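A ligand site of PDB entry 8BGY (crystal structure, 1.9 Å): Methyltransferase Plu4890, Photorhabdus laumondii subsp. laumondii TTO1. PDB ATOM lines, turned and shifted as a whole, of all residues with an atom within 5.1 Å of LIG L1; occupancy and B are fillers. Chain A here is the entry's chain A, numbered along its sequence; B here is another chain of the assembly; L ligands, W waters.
An oxygen (O4) of LIG L1 sits close to the side-chain sulfur (SD) of Met 259 (3.5 Å). Phe 85 touches LIG L1. OH of Tyr 98 touches C1 of LIG L1, at 3.2 Å. Phe 140 touches LIG L1. Leu 143 touches LIG L1. Met 144 touches LIG L1. Val 147 touches LIG L1 (CG1 to C10, 3.9 Å). Asn 227 touches LIG L1 (O to C16, 3.2 Å). His 230 touches LIG L1 (CE1 to C16, 3.7 Å). Phe 269 touches LIG L1. Leu 272 touches LIG L1. Met 273 touches LIG L1 (CE to C3, 3.7 Å). Leu 276 touches LIG L1 (CD1 to C1, 3.3 Å). CE1 of Tyr 308 touches C9 of LIG L1 (3.7 Å). 16 residues have an atom within 4 Å of LIG L1: Phe 85, Met 89, Tyr 98, Phe 140, Leu 143, Met 144, Val 147, Asn 227, His 230, Asn 231, Met 259, Phe 269, Leu 272, Met 273, Leu 276 and Tyr 308.
The side-chain amide oxygen of Asn 227 is in hydrogen-bond range of a ring nitrogen (NE2) of His 230, 3.3 Å away. The backbone NH of Met 259 is in hydrogen-bond range of the side-chain amide oxygen of Asn 227, 3.2 Å away. SD of Met 273 lies within hydrogen-bond range of ND2 of Asn 231, at 3.7 Å. OH of Tyr 311 is in hydrogen-bond range of OH of Tyr 308 (2.6 Å). The side-chain amide nitrogen (ND2) of Asn 227 sits at hydrogen-bond distance from the side-chain hydroxyl (OH) of Tyr 311, at 2.7 Å.
The side-chain amide nitrogen (ND2) of Asn 231 sits at hydrogen-bond distance from an oxygen (O5) of LIG L1 (2.9 Å). The side-chain sulfur (SD) of Met 89 lies close to an oxygen (O3) of LIG L1 (3.6 Å).
Water W2 lies within hydrogen-bond range of an oxygen (O2) of LIG L1 (2.7 Å) and the side-chain hydroxyl of Tyr 98 (3.1 Å). Water W1 lies within hydrogen-bond range of the guanidinium group of Arg 11 of chain B (2.9 Å) and an oxygen (O3) of LIG L1 (3.5 Å).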
ATOM      1  N   PHE A  85     -26.760 -15.883  13.429  1.00  0.00           N
ATOM      2  CA  PHE A  85     -26.865 -15.174  12.125  1.00  0.00           C
ATOM      3  C   PHE A  85     -26.671 -16.183  10.983  1.00  0.00           C
ATOM      4  O   PHE A  85     -27.269 -15.996   9.909  1.00  0.00           O
ATOM      5  CB  PHE A  85     -25.896 -13.994  12.062  1.00  0.00           C
ATOM      6  CG  PHE A  85     -24.571 -14.264  11.376  1.00  0.00           C
ATOM      7  CD1 PHE A  85     -24.483 -14.284   9.988  1.00  0.00           C
ATOM      8  CD2 PHE A  85     -23.423 -14.468  12.118  1.00  0.00           C
ATOM      9  CE1 PHE A  85     -23.266 -14.516   9.366  1.00  0.00           C
ATOM     10  CE2 PHE A  85     -22.202 -14.697  11.487  1.00  0.00           C
ATOM     11  CZ  PHE A  85     -22.130 -14.731  10.111  1.00  0.00           C
ATOM     12  N   MET A  89     -28.882 -16.922   7.657  1.00  0.00           N
ATOM     13  CA  MET A  89     -28.111 -16.774   6.385  1.00  0.00           C
ATOM     14  C   MET A  89     -28.504 -17.893   5.415  1.00  0.00           C
ATOM     15  O   MET A  89     -28.921 -17.571   4.287  1.00  0.00           O
ATOM     16  CB  MET A  89     -26.602 -16.805   6.628  1.00  0.00           C
ATOM     17  CG  MET A  89     -25.790 -16.577   5.361  1.00  0.00           C
ATOM     18  SD  MET A  89     -24.010 -16.624   5.642  1.00  0.00           S
ATOM     19  CE  MET A  89     -23.403 -16.439   3.958  1.00  0.00           C
ATOM     20  N   GLU A  93     -30.122 -17.869   1.811  1.00  0.00           N
ATOM     21  CA  GLU A  93     -29.078 -18.082   0.768  1.00  0.00           C
ATOM     22  C   GLU A  93     -29.670 -18.805  -0.451  1.00  0.00           C
ATOM     23  O   GLU A  93     -29.497 -18.285  -1.571  1.00  0.00           O
ATOM     24  CB  GLU A  93     -27.890 -18.873   1.333  1.00  0.00           C
ATOM     25  CG  GLU A  93     -26.678 -18.877   0.429  1.00  0.00           C
ATOM     26  CD  GLU A  93     -26.028 -17.525   0.207  1.00  0.00           C
ATOM     27  OE1 GLU A  93     -26.034 -16.701   1.145  1.00  0.00           O
ATOM     28  OE2 GLU A  93     -25.517 -17.295  -0.915  1.00  0.00           O
ATOM     29  N   TYR A  98     -34.222 -16.001  -3.915  1.00  0.00           N
ATOM     30  CA  TYR A  98     -32.761 -15.804  -4.175  1.00  0.00           C
ATOM     31  C   TYR A  98     -32.357 -16.626  -5.412  1.00  0.00           C
ATOM     32  O   TYR A  98     -31.721 -16.070  -6.329  1.00  0.00           O
ATOM     33  CB  TYR A  98     -31.927 -16.178  -2.951  1.00  0.00           C
ATOM     34  CG  TYR A  98     -31.793 -15.103  -1.902  1.00  0.00           C
ATOM     35  CD1 TYR A  98     -30.562 -14.798  -1.350  1.00  0.00           C
ATOM     36  CD2 TYR A  98     -32.903 -14.388  -1.460  1.00  0.00           C
ATOM     37  CE1 TYR A  98     -30.431 -13.815  -0.374  1.00  0.00           C
ATOM     38  CE2 TYR A  98     -32.792 -13.411  -0.492  1.00  0.00           C
ATOM     39  CZ  TYR A  98     -31.549 -13.115   0.050  1.00  0.00           C
ATOM     40  OH  TYR A  98     -31.435 -12.145   1.006  1.00  0.00           O
ATOM     41  N   PHE A 126     -35.839  -5.265  -4.393  1.00  0.00           N
ATOM     42  CA  PHE A 126     -35.706  -6.176  -3.218  1.00  0.00           C
ATOM     43  C   PHE A 126     -36.569  -5.688  -2.044  1.00  0.00           C
ATOM     44  O   PHE A 126     -37.475  -6.433  -1.609  1.00  0.00           O
ATOM     45  CB  PHE A 126     -34.238  -6.294  -2.795  1.00  0.00           C
ATOM     46  CG  PHE A 126     -33.965  -7.324  -1.732  1.00  0.00           C
ATOM     47  CD1 PHE A 126     -33.813  -8.667  -2.061  1.00  0.00           C
ATOM     48  CD2 PHE A 126     -33.861  -6.947  -0.403  1.00  0.00           C
ATOM     49  CE1 PHE A 126     -33.559  -9.608  -1.075  1.00  0.00           C
ATOM     50  CE2 PHE A 126     -33.607  -7.897   0.580  1.00  0.00           C
ATOM     51  CZ  PHE A 126     -33.461  -9.217   0.246  1.00  0.00           C
ATOM     52  N   PHE A 127     -36.305  -4.474  -1.545  1.00  0.00           N
ATOM     53  CA  PHE A 127     -36.891  -3.933  -0.288  1.00  0.00           C
ATOM     54  C   PHE A 127     -38.398  -3.672  -0.461  1.00  0.00           C
ATOM     55  O   PHE A 127     -39.149  -3.912   0.505  1.00  0.00           O
ATOM     56  CB  PHE A 127     -36.127  -2.687   0.161  1.00  0.00           C
ATOM     57  CG  PHE A 127     -34.762  -2.989   0.713  1.00  0.00           C
ATOM     58  CD1 PHE A 127     -34.611  -3.800   1.837  1.00  0.00           C
ATOM     59  CD2 PHE A 127     -33.615  -2.479   0.120  1.00  0.00           C
ATOM     60  CE1 PHE A 127     -33.358  -4.092   2.345  1.00  0.00           C
ATOM     61  CE2 PHE A 127     -32.361  -2.762   0.631  1.00  0.00           C
ATOM     62  CZ  PHE A 127     -32.240  -3.569   1.747  1.00  0.00           C
ATOM     63  N   PHE A 140     -34.591 -11.648   6.839  1.00  0.00           N
ATOM     64  CA  PHE A 140     -33.572 -10.635   6.436  1.00  0.00           C
ATOM     65  C   PHE A 140     -33.326  -9.665   7.597  1.00  0.00           C
ATOM     66  O   PHE A 140     -32.151  -9.454   7.961  1.00  0.00           O
ATOM     67  CB  PHE A 140     -33.995  -9.872   5.177  1.00  0.00           C
ATOM     68  CG  PHE A 140     -33.018  -8.792   4.770  1.00  0.00           C
ATOM     69  CD1 PHE A 140     -31.900  -9.103   4.015  1.00  0.00           C
ATOM     70  CD2 PHE A 140     -33.206  -7.482   5.174  1.00  0.00           C
ATOM     71  CE1 PHE A 140     -30.991  -8.119   3.655  1.00  0.00           C
ATOM     72  CE2 PHE A 140     -32.298  -6.499   4.814  1.00  0.00           C
ATOM     73  CZ  PHE A 140     -31.190  -6.817   4.054  1.00  0.00           C
ATOM     74  N   LEU A 143     -31.427 -11.373  10.307  1.00  0.00           N
ATOM     75  CA  LEU A 143     -30.007 -11.518   9.907  1.00  0.00           C
ATOM     76  C   LEU A 143     -29.253 -10.210  10.198  1.00  0.00           C
ATOM     77  O   LEU A 143     -28.165 -10.285  10.807  1.00  0.00           O
ATOM     78  CB  LEU A 143     -29.931 -11.885   8.421  1.00  0.00           C
ATOM     79  CG  LEU A 143     -28.531 -12.031   7.829  1.00  0.00           C
ATOM     80  CD1 LEU A 143     -27.739 -13.111   8.539  1.00  0.00           C
ATOM     81  CD2 LEU A 143     -28.597 -12.314   6.333  1.00  0.00           C
ATOM     82  N   MET A 144     -29.816  -9.070   9.786  1.00  0.00           N
ATOM     83  CA  MET A 144     -29.235  -7.709   9.972  1.00  0.00           C
ATOM     84  C   MET A 144     -29.105  -7.409  11.471  1.00  0.00           C
ATOM     85  O   MET A 144     -28.084  -6.822  11.867  1.00  0.00           O
ATOM     86  CB  MET A 144     -30.095  -6.632   9.315  1.00  0.00           C
ATOM     87  CG  MET A 144     -30.180  -6.737   7.790  1.00  0.00           C
ATOM     88  SD  MET A 144     -28.562  -6.811   6.973  1.00  0.00           S
ATOM     89  CE  MET A 144     -28.353  -8.584   6.827  1.00  0.00           C
ATOM     90  N   VAL A 147     -26.044  -9.606  13.026  1.00  0.00           N
ATOM     91  CA  VAL A 147     -24.702  -9.070  12.612  1.00  0.00           C
ATOM     92  C   VAL A 147     -24.480  -7.703  13.264  1.00  0.00           C
ATOM     93  O   VAL A 147     -23.320  -7.404  13.617  1.00  0.00           O
ATOM     94  CB  VAL A 147     -24.541  -9.005  11.077  1.00  0.00           C
ATOM     95  CG1 VAL A 147     -24.576 -10.401  10.454  1.00  0.00           C
ATOM     96  CG2 VAL A 147     -25.557  -8.094  10.407  1.00  0.00           C
ATOM     97  N   ASN A 227     -23.910  -0.770   6.531  1.00  0.00           N
ATOM     98  CA  ASN A 227     -24.291  -1.794   5.528  1.00  0.00           C
ATOM     99  C   ASN A 227     -25.532  -1.344   4.755  1.00  0.00           C
ATOM    100  O   ASN A 227     -26.537  -2.080   4.756  1.00  0.00           O
ATOM    101  CB  ASN A 227     -24.508  -3.170   6.177  1.00  0.00           C
ATOM    102  CG  ASN A 227     -23.243  -3.812   6.691  1.00  0.00           C
ATOM    103  OD1 ASN A 227     -22.144  -3.478   6.259  1.00  0.00           O
ATOM    104  ND2 ASN A 227     -23.381  -4.745   7.620  1.00  0.00           N
ATOM    105  N   HIS A 230     -23.907  -0.655  -0.200  1.00  0.00           N
ATOM    106  CA  HIS A 230     -23.675  -1.817  -1.104  1.00  0.00           C
ATOM    107  C   HIS A 230     -25.016  -2.400  -1.590  1.00  0.00           C
ATOM    108  O   HIS A 230     -24.991  -3.451  -2.252  1.00  0.00           O
ATOM    109  CB  HIS A 230     -22.740  -2.876  -0.483  1.00  0.00           C
ATOM    110  CG  HIS A 230     -23.007  -3.245   0.937  1.00  0.00           C
ATOM    111  ND1 HIS A 230     -24.222  -3.723   1.376  1.00  0.00           N
ATOM    112  CD2 HIS A 230     -22.183  -3.244   2.010  1.00  0.00           C
ATOM    113  CE1 HIS A 230     -24.153  -3.973   2.667  1.00  0.00           C
ATOM    114  NE2 HIS A 230     -22.907  -3.696   3.073  1.00  0.00           N
ATOM    115  N   ASN A 231     -26.143  -1.731  -1.298  1.00  0.00           N
ATOM    116  CA  ASN A 231     -27.476  -2.018  -1.888  1.00  0.00           C
ATOM    117  C   ASN A 231     -27.791  -0.995  -2.989  1.00  0.00           C
ATOM    118  O   ASN A 231     -28.889  -1.095  -3.578  1.00  0.00           O
ATOM    119  CB  ASN A 231     -28.596  -1.979  -0.846  1.00  0.00           C
ATOM    120  CG  ASN A 231     -28.361  -2.879   0.343  1.00  0.00           C
ATOM    121  OD1 ASN A 231     -28.803  -2.572   1.455  1.00  0.00           O
ATOM    122  ND2 ASN A 231     -27.689  -4.005   0.138  1.00  0.00           N
ATOM    123  N   MET A 259     -19.089  -3.566   5.350  1.00  0.00           N
ATOM    124  CA  MET A 259     -18.276  -4.721   4.885  1.00  0.00           C
ATOM    125  C   MET A 259     -17.464  -4.237   3.674  1.00  0.00           C
ATOM    126  O   MET A 259     -18.094  -3.822   2.682  1.00  0.00           O
ATOM    127  CB  MET A 259     -19.160  -5.902   4.450  1.00  0.00           C
ATOM    128  CG  MET A 259     -19.924  -6.546   5.595  1.00  0.00           C
ATOM    129  SD  MET A 259     -21.153  -7.733   5.004  1.00  0.00           S
ATOM    130  CE  MET A 259     -22.318  -6.629   4.214  1.00  0.00           C
ATOM    131  N   PHE A 269     -19.814 -12.098  -2.372  1.00  0.00           N
ATOM    132  CA  PHE A 269     -20.789 -11.137  -1.800  1.00  0.00           C
ATOM    133  C   PHE A 269     -21.015  -9.970  -2.773  1.00  0.00           C
ATOM    134  O   PHE A 269     -22.158  -9.518  -2.913  1.00  0.00           O
ATOM    135  CB  PHE A 269     -20.330 -10.622  -0.435  1.00  0.00           C
ATOM    136  CG  PHE A 269     -21.358  -9.746   0.247  1.00  0.00           C
ATOM    137  CD1 PHE A 269     -22.424 -10.312   0.936  1.00  0.00           C
ATOM    138  CD2 PHE A 269     -21.270  -8.363   0.183  1.00  0.00           C
ATOM    139  CE1 PHE A 269     -23.372  -9.514   1.554  1.00  0.00           C
ATOM    140  CE2 PHE A 269     -22.218  -7.565   0.801  1.00  0.00           C
ATOM    141  CZ  PHE A 269     -23.263  -8.140   1.483  1.00  0.00           C
ATOM    142  N   LEU A 272     -23.496 -11.122  -5.295  1.00  0.00           N
ATOM    143  CA  LEU A 272     -24.840 -11.227  -4.653  1.00  0.00           C
ATOM    144  C   LEU A 272     -25.503  -9.846  -4.618  1.00  0.00           C
ATOM    145  O   LEU A 272     -26.715  -9.787  -4.900  1.00  0.00           O
ATOM    146  CB  LEU A 272     -24.695 -11.804  -3.241  1.00  0.00           C
ATOM    147  CG  LEU A 272     -26.001 -11.956  -2.458  1.00  0.00           C
ATOM    148  CD1 LEU A 272     -26.901 -13.004  -3.109  1.00  0.00           C
ATOM    149  CD2 LEU A 272     -25.731 -12.322  -1.008  1.00  0.00           C
ATOM    150  N   MET A 273     -24.745  -8.804  -4.288  1.00  0.00           N
ATOM    151  CA  MET A 273     -25.232  -7.397  -4.233  1.00  0.00           C
ATOM    152  C   MET A 273     -25.660  -6.936  -5.628  1.00  0.00           C
ATOM    153  O   MET A 273     -26.634  -6.160  -5.725  1.00  0.00           O
ATOM    154  CB  MET A 273     -24.160  -6.450  -3.689  1.00  0.00           C
ATOM    155  CG  MET A 273     -23.832  -6.658  -2.215  1.00  0.00           C
ATOM    156  SD  MET A 273     -25.285  -6.585  -1.127  1.00  0.00           S
ATOM    157  CE  MET A 273     -25.701  -8.327  -1.004  1.00  0.00           C
ATOM    158  N   LEU A 276     -29.148  -8.902  -6.403  1.00  0.00           N
ATOM    159  CA  LEU A 276     -30.297  -8.521  -5.538  1.00  0.00           C
ATOM    160  C   LEU A 276     -30.639  -7.032  -5.697  1.00  0.00           C
ATOM    161  O   LEU A 276     -31.849  -6.718  -5.594  1.00  0.00           O
ATOM    162  CB  LEU A 276     -29.985  -8.870  -4.080  1.00  0.00           C
ATOM    163  CG  LEU A 276     -29.840 -10.363  -3.779  1.00  0.00           C
ATOM    164  CD1 LEU A 276     -29.503 -10.581  -2.305  1.00  0.00           C
ATOM    165  CD2 LEU A 276     -31.103 -11.126  -4.142  1.00  0.00           C
ATOM    166  N   PHE A 277     -29.660  -6.161  -5.916  1.00  0.00           N
ATOM    167  CA  PHE A 277     -29.814  -4.683  -5.777  1.00  0.00           C
ATOM    168  C   PHE A 277     -29.229  -3.883  -6.953  1.00  0.00           C
ATOM    169  O   PHE A 277     -29.512  -2.671  -7.013  1.00  0.00           O
ATOM    170  CB  PHE A 277     -29.125  -4.203  -4.503  1.00  0.00           C
ATOM    171  CG  PHE A 277     -29.602  -4.872  -3.230  1.00  0.00           C
ATOM    172  CD1 PHE A 277     -30.811  -4.529  -2.660  1.00  0.00           C
ATOM    173  CD2 PHE A 277     -28.832  -5.847  -2.615  1.00  0.00           C
ATOM    174  CE1 PHE A 277     -31.240  -5.134  -1.494  1.00  0.00           C
ATOM    175  CE2 PHE A 277     -29.264  -6.464  -1.443  1.00  0.00           C
ATOM    176  CZ  PHE A 277     -30.476  -6.105  -0.890  1.00  0.00           C
ATOM    177  N   TYR A 308     -16.842 -13.114   9.649  1.00  0.00           N
ATOM    178  CA  TYR A 308     -17.331 -13.404   8.278  1.00  0.00           C
ATOM    179  C   TYR A 308     -16.741 -12.439   7.242  1.00  0.00           C
ATOM    180  O   TYR A 308     -16.657 -12.830   6.056  1.00  0.00           O
ATOM    181  CB  TYR A 308     -18.865 -13.373   8.235  1.00  0.00           C
ATOM    182  CG  TYR A 308     -19.505 -12.082   8.675  1.00  0.00           C
ATOM    183  CD1 TYR A 308     -19.740 -11.055   7.777  1.00  0.00           C
ATOM    184  CD2 TYR A 308     -19.874 -11.888   9.994  1.00  0.00           C
ATOM    185  CE1 TYR A 308     -20.333  -9.870   8.178  1.00  0.00           C
ATOM    186  CE2 TYR A 308     -20.460 -10.707  10.408  1.00  0.00           C
ATOM    187  CZ  TYR A 308     -20.692  -9.686   9.497  1.00  0.00           C
ATOM    188  OH  TYR A 308     -21.280  -8.525   9.904  1.00  0.00           O
ATOM    189  N   TYR A 311     -14.566  -5.012   8.060  1.00  0.00           N
ATOM    190  CA  TYR A 311     -15.429  -3.804   8.010  1.00  0.00           C
ATOM    191  C   TYR A 311     -14.547  -2.549   7.888  1.00  0.00           C
ATOM    192  O   TYR A 311     -13.485  -2.508   8.535  1.00  0.00           O
ATOM    193  CB  TYR A 311     -16.305  -3.707   9.258  1.00  0.00           C
ATOM    194  CG  TYR A 311     -17.656  -4.369   9.149  1.00  0.00           C
ATOM    195  CD1 TYR A 311     -18.815  -3.618   9.029  1.00  0.00           C
ATOM    196  CD2 TYR A 311     -17.784  -5.756   9.166  1.00  0.00           C
ATOM    197  CE1 TYR A 311     -20.066  -4.224   8.926  1.00  0.00           C
ATOM    198  CE2 TYR A 311     -19.025  -6.373   9.062  1.00  0.00           C
ATOM    199  CZ  TYR A 311     -20.161  -5.603   8.945  1.00  0.00           C
ATOM    200  OH  TYR A 311     -21.389  -6.190   8.843  1.00  0.00           O
ATOM    201  N   ARG B  11     -23.243 -19.676  -4.675  1.00  0.00           N
ATOM    202  CA  ARG B  11     -22.848 -18.469  -5.449  1.00  0.00           C
ATOM    203  C   ARG B  11     -21.828 -18.848  -6.529  1.00  0.00           C
ATOM    204  O   ARG B  11     -21.841 -18.210  -7.595  1.00  0.00           O
ATOM    205  CB  ARG B  11     -22.281 -17.387  -4.522  1.00  0.00           C
ATOM    206  CG  ARG B  11     -23.256 -16.887  -3.468  1.00  0.00           C
ATOM    207  CD  ARG B  11     -22.660 -15.777  -2.633  1.00  0.00           C
ATOM    208  NE  ARG B  11     -23.423 -15.531  -1.413  1.00  0.00           N
ATOM    209  CZ  ARG B  11     -23.021 -14.764  -0.395  1.00  0.00           C
ATOM    210  NH1 ARG B  11     -23.788 -14.625   0.671  1.00  0.00           N
ATOM    211  NH2 ARG B  11     -21.842 -14.148  -0.442  1.00  0.00           N
HETATM  212  C1  LIG L   1     -28.867 -10.249   0.940  1.00  0.00           C
HETATM  213  O1  LIG L   1     -27.705 -10.427   1.760  1.00  0.00           O
HETATM  214  C2  LIG L   1     -27.239  -9.347   2.446  1.00  0.00           C
HETATM  215  C3  LIG L   1     -27.598  -8.031   2.143  1.00  0.00           C
HETATM  216  C4  LIG L   1     -26.356  -9.610   3.512  1.00  0.00           C
HETATM  217  C5  LIG L   1     -25.988 -10.926   3.818  1.00  0.00           C
HETATM  218  O2  LIG L   1     -26.438 -11.875   3.178  1.00  0.00           O
HETATM  219  C6  LIG L   1     -25.111 -11.166   4.878  1.00  0.00           C
HETATM  220  C7  LIG L   1     -24.726 -12.470   5.205  1.00  0.00           C
HETATM  221  O3  LIG L   1     -25.251 -13.477   4.467  1.00  0.00           O
HETATM  222  C8  LIG L   1     -23.860 -12.727   6.256  1.00  0.00           C
HETATM  223  C9  LIG L   1     -23.348 -11.666   6.995  1.00  0.00           C
HETATM  224  C10 LIG L   1     -23.714 -10.356   6.676  1.00  0.00           C
HETATM  225  C11 LIG L   1     -24.590 -10.097   5.622  1.00  0.00           C
HETATM  226  C12 LIG L   1     -24.958  -8.790   5.313  1.00  0.00           C
HETATM  227  O4  LIG L   1     -24.506  -7.848   5.974  1.00  0.00           O
HETATM  228  C13 LIG L   1     -25.836  -8.550   4.253  1.00  0.00           C
HETATM  229  C14 LIG L   1     -26.201  -7.230   3.938  1.00  0.00           C
HETATM  230  C15 LIG L   1     -27.090  -6.982   2.887  1.00  0.00           C
HETATM  231  O5  LIG L   1     -27.479  -5.726   2.512  1.00  0.00           O
HETATM  232  C16 LIG L   1     -27.717  -4.729   3.505  1.00  0.00           C
HETATM  233  N1  LG2 L   2     -28.191  -0.724   9.047  1.00  0.00           N
HETATM  234  C1  LG2 L   2     -28.764  -2.071   9.371  1.00  0.00           C
HETATM  235  C2  LG2 L   2     -29.613  -2.614   8.224  1.00  0.00           C
HETATM  236  C3  LG2 L   2     -28.869  -2.689   6.897  1.00  0.00           C
HETATM  237  S1  LG2 L   2     -29.859  -3.446   5.584  1.00  0.00           S
HETATM  238  C4  LG2 L   2     -27.626  -3.049   9.677  1.00  0.00           C
HETATM  239  O1  LG2 L   2     -27.840  -4.115  10.246  1.00  0.00           O
HETATM  240  O2  LG2 L   2     -26.465  -2.788   9.362  1.00  0.00           O
HETATM  241  C5  LG2 L   2     -30.399  -1.999   4.640  1.00  0.00           C
HETATM  242  C6  LG2 L   2     -31.534  -1.258   5.301  1.00  0.00           C
HETATM  243  O3  LG2 L   2     -31.883  -0.100   4.504  1.00  0.00           O
HETATM  244  C7  LG2 L   2     -32.827  -2.075   5.469  1.00  0.00           C
HETATM  245  O4  LG2 L   2     -33.267  -2.033   6.817  1.00  0.00           O
HETATM  246  C8  LG2 L   2     -33.821  -1.375   4.534  1.00  0.00           C
HETATM  247  O5  LG2 L   2     -35.152  -1.443   4.996  1.00  0.00           O
HETATM  248  C9  LG2 L   2     -33.288   0.054   4.550  1.00  0.00           C
HETATM  249  N2  LG2 L   2     -33.708   0.871   3.419  1.00  0.00           N
HETATM  250  C10 LG2 L   2     -33.739   0.510   2.096  1.00  0.00           C
HETATM  251  N3  LG2 L   2     -34.159   1.461   1.301  1.00  0.00           N
HETATM  252  C11 LG2 L   2     -34.413   2.524   2.156  1.00  0.00           C
HETATM  253  C12 LG2 L   2     -34.886   3.833   1.924  1.00  0.00           C
HETATM  254  N4  LG2 L   2     -35.186   4.311   0.716  1.00  0.00           N
HETATM  255  N5  LG2 L   2     -35.027   4.641   2.999  1.00  0.00           N
HETATM  256  C13 LG2 L   2     -34.730   4.160   4.216  1.00  0.00           C
HETATM  257  N6  LG2 L   2     -34.281   2.956   4.550  1.00  0.00           N
HETATM  258  C14 LG2 L   2     -34.145   2.172   3.468  1.00  0.00           C
HETATM  259  O   HOH W   1     -22.240 -13.361   2.765  1.00  0.00           O
HETATM  260  O   HOH W   2     -28.850 -12.968   2.521  1.00  0.00           O
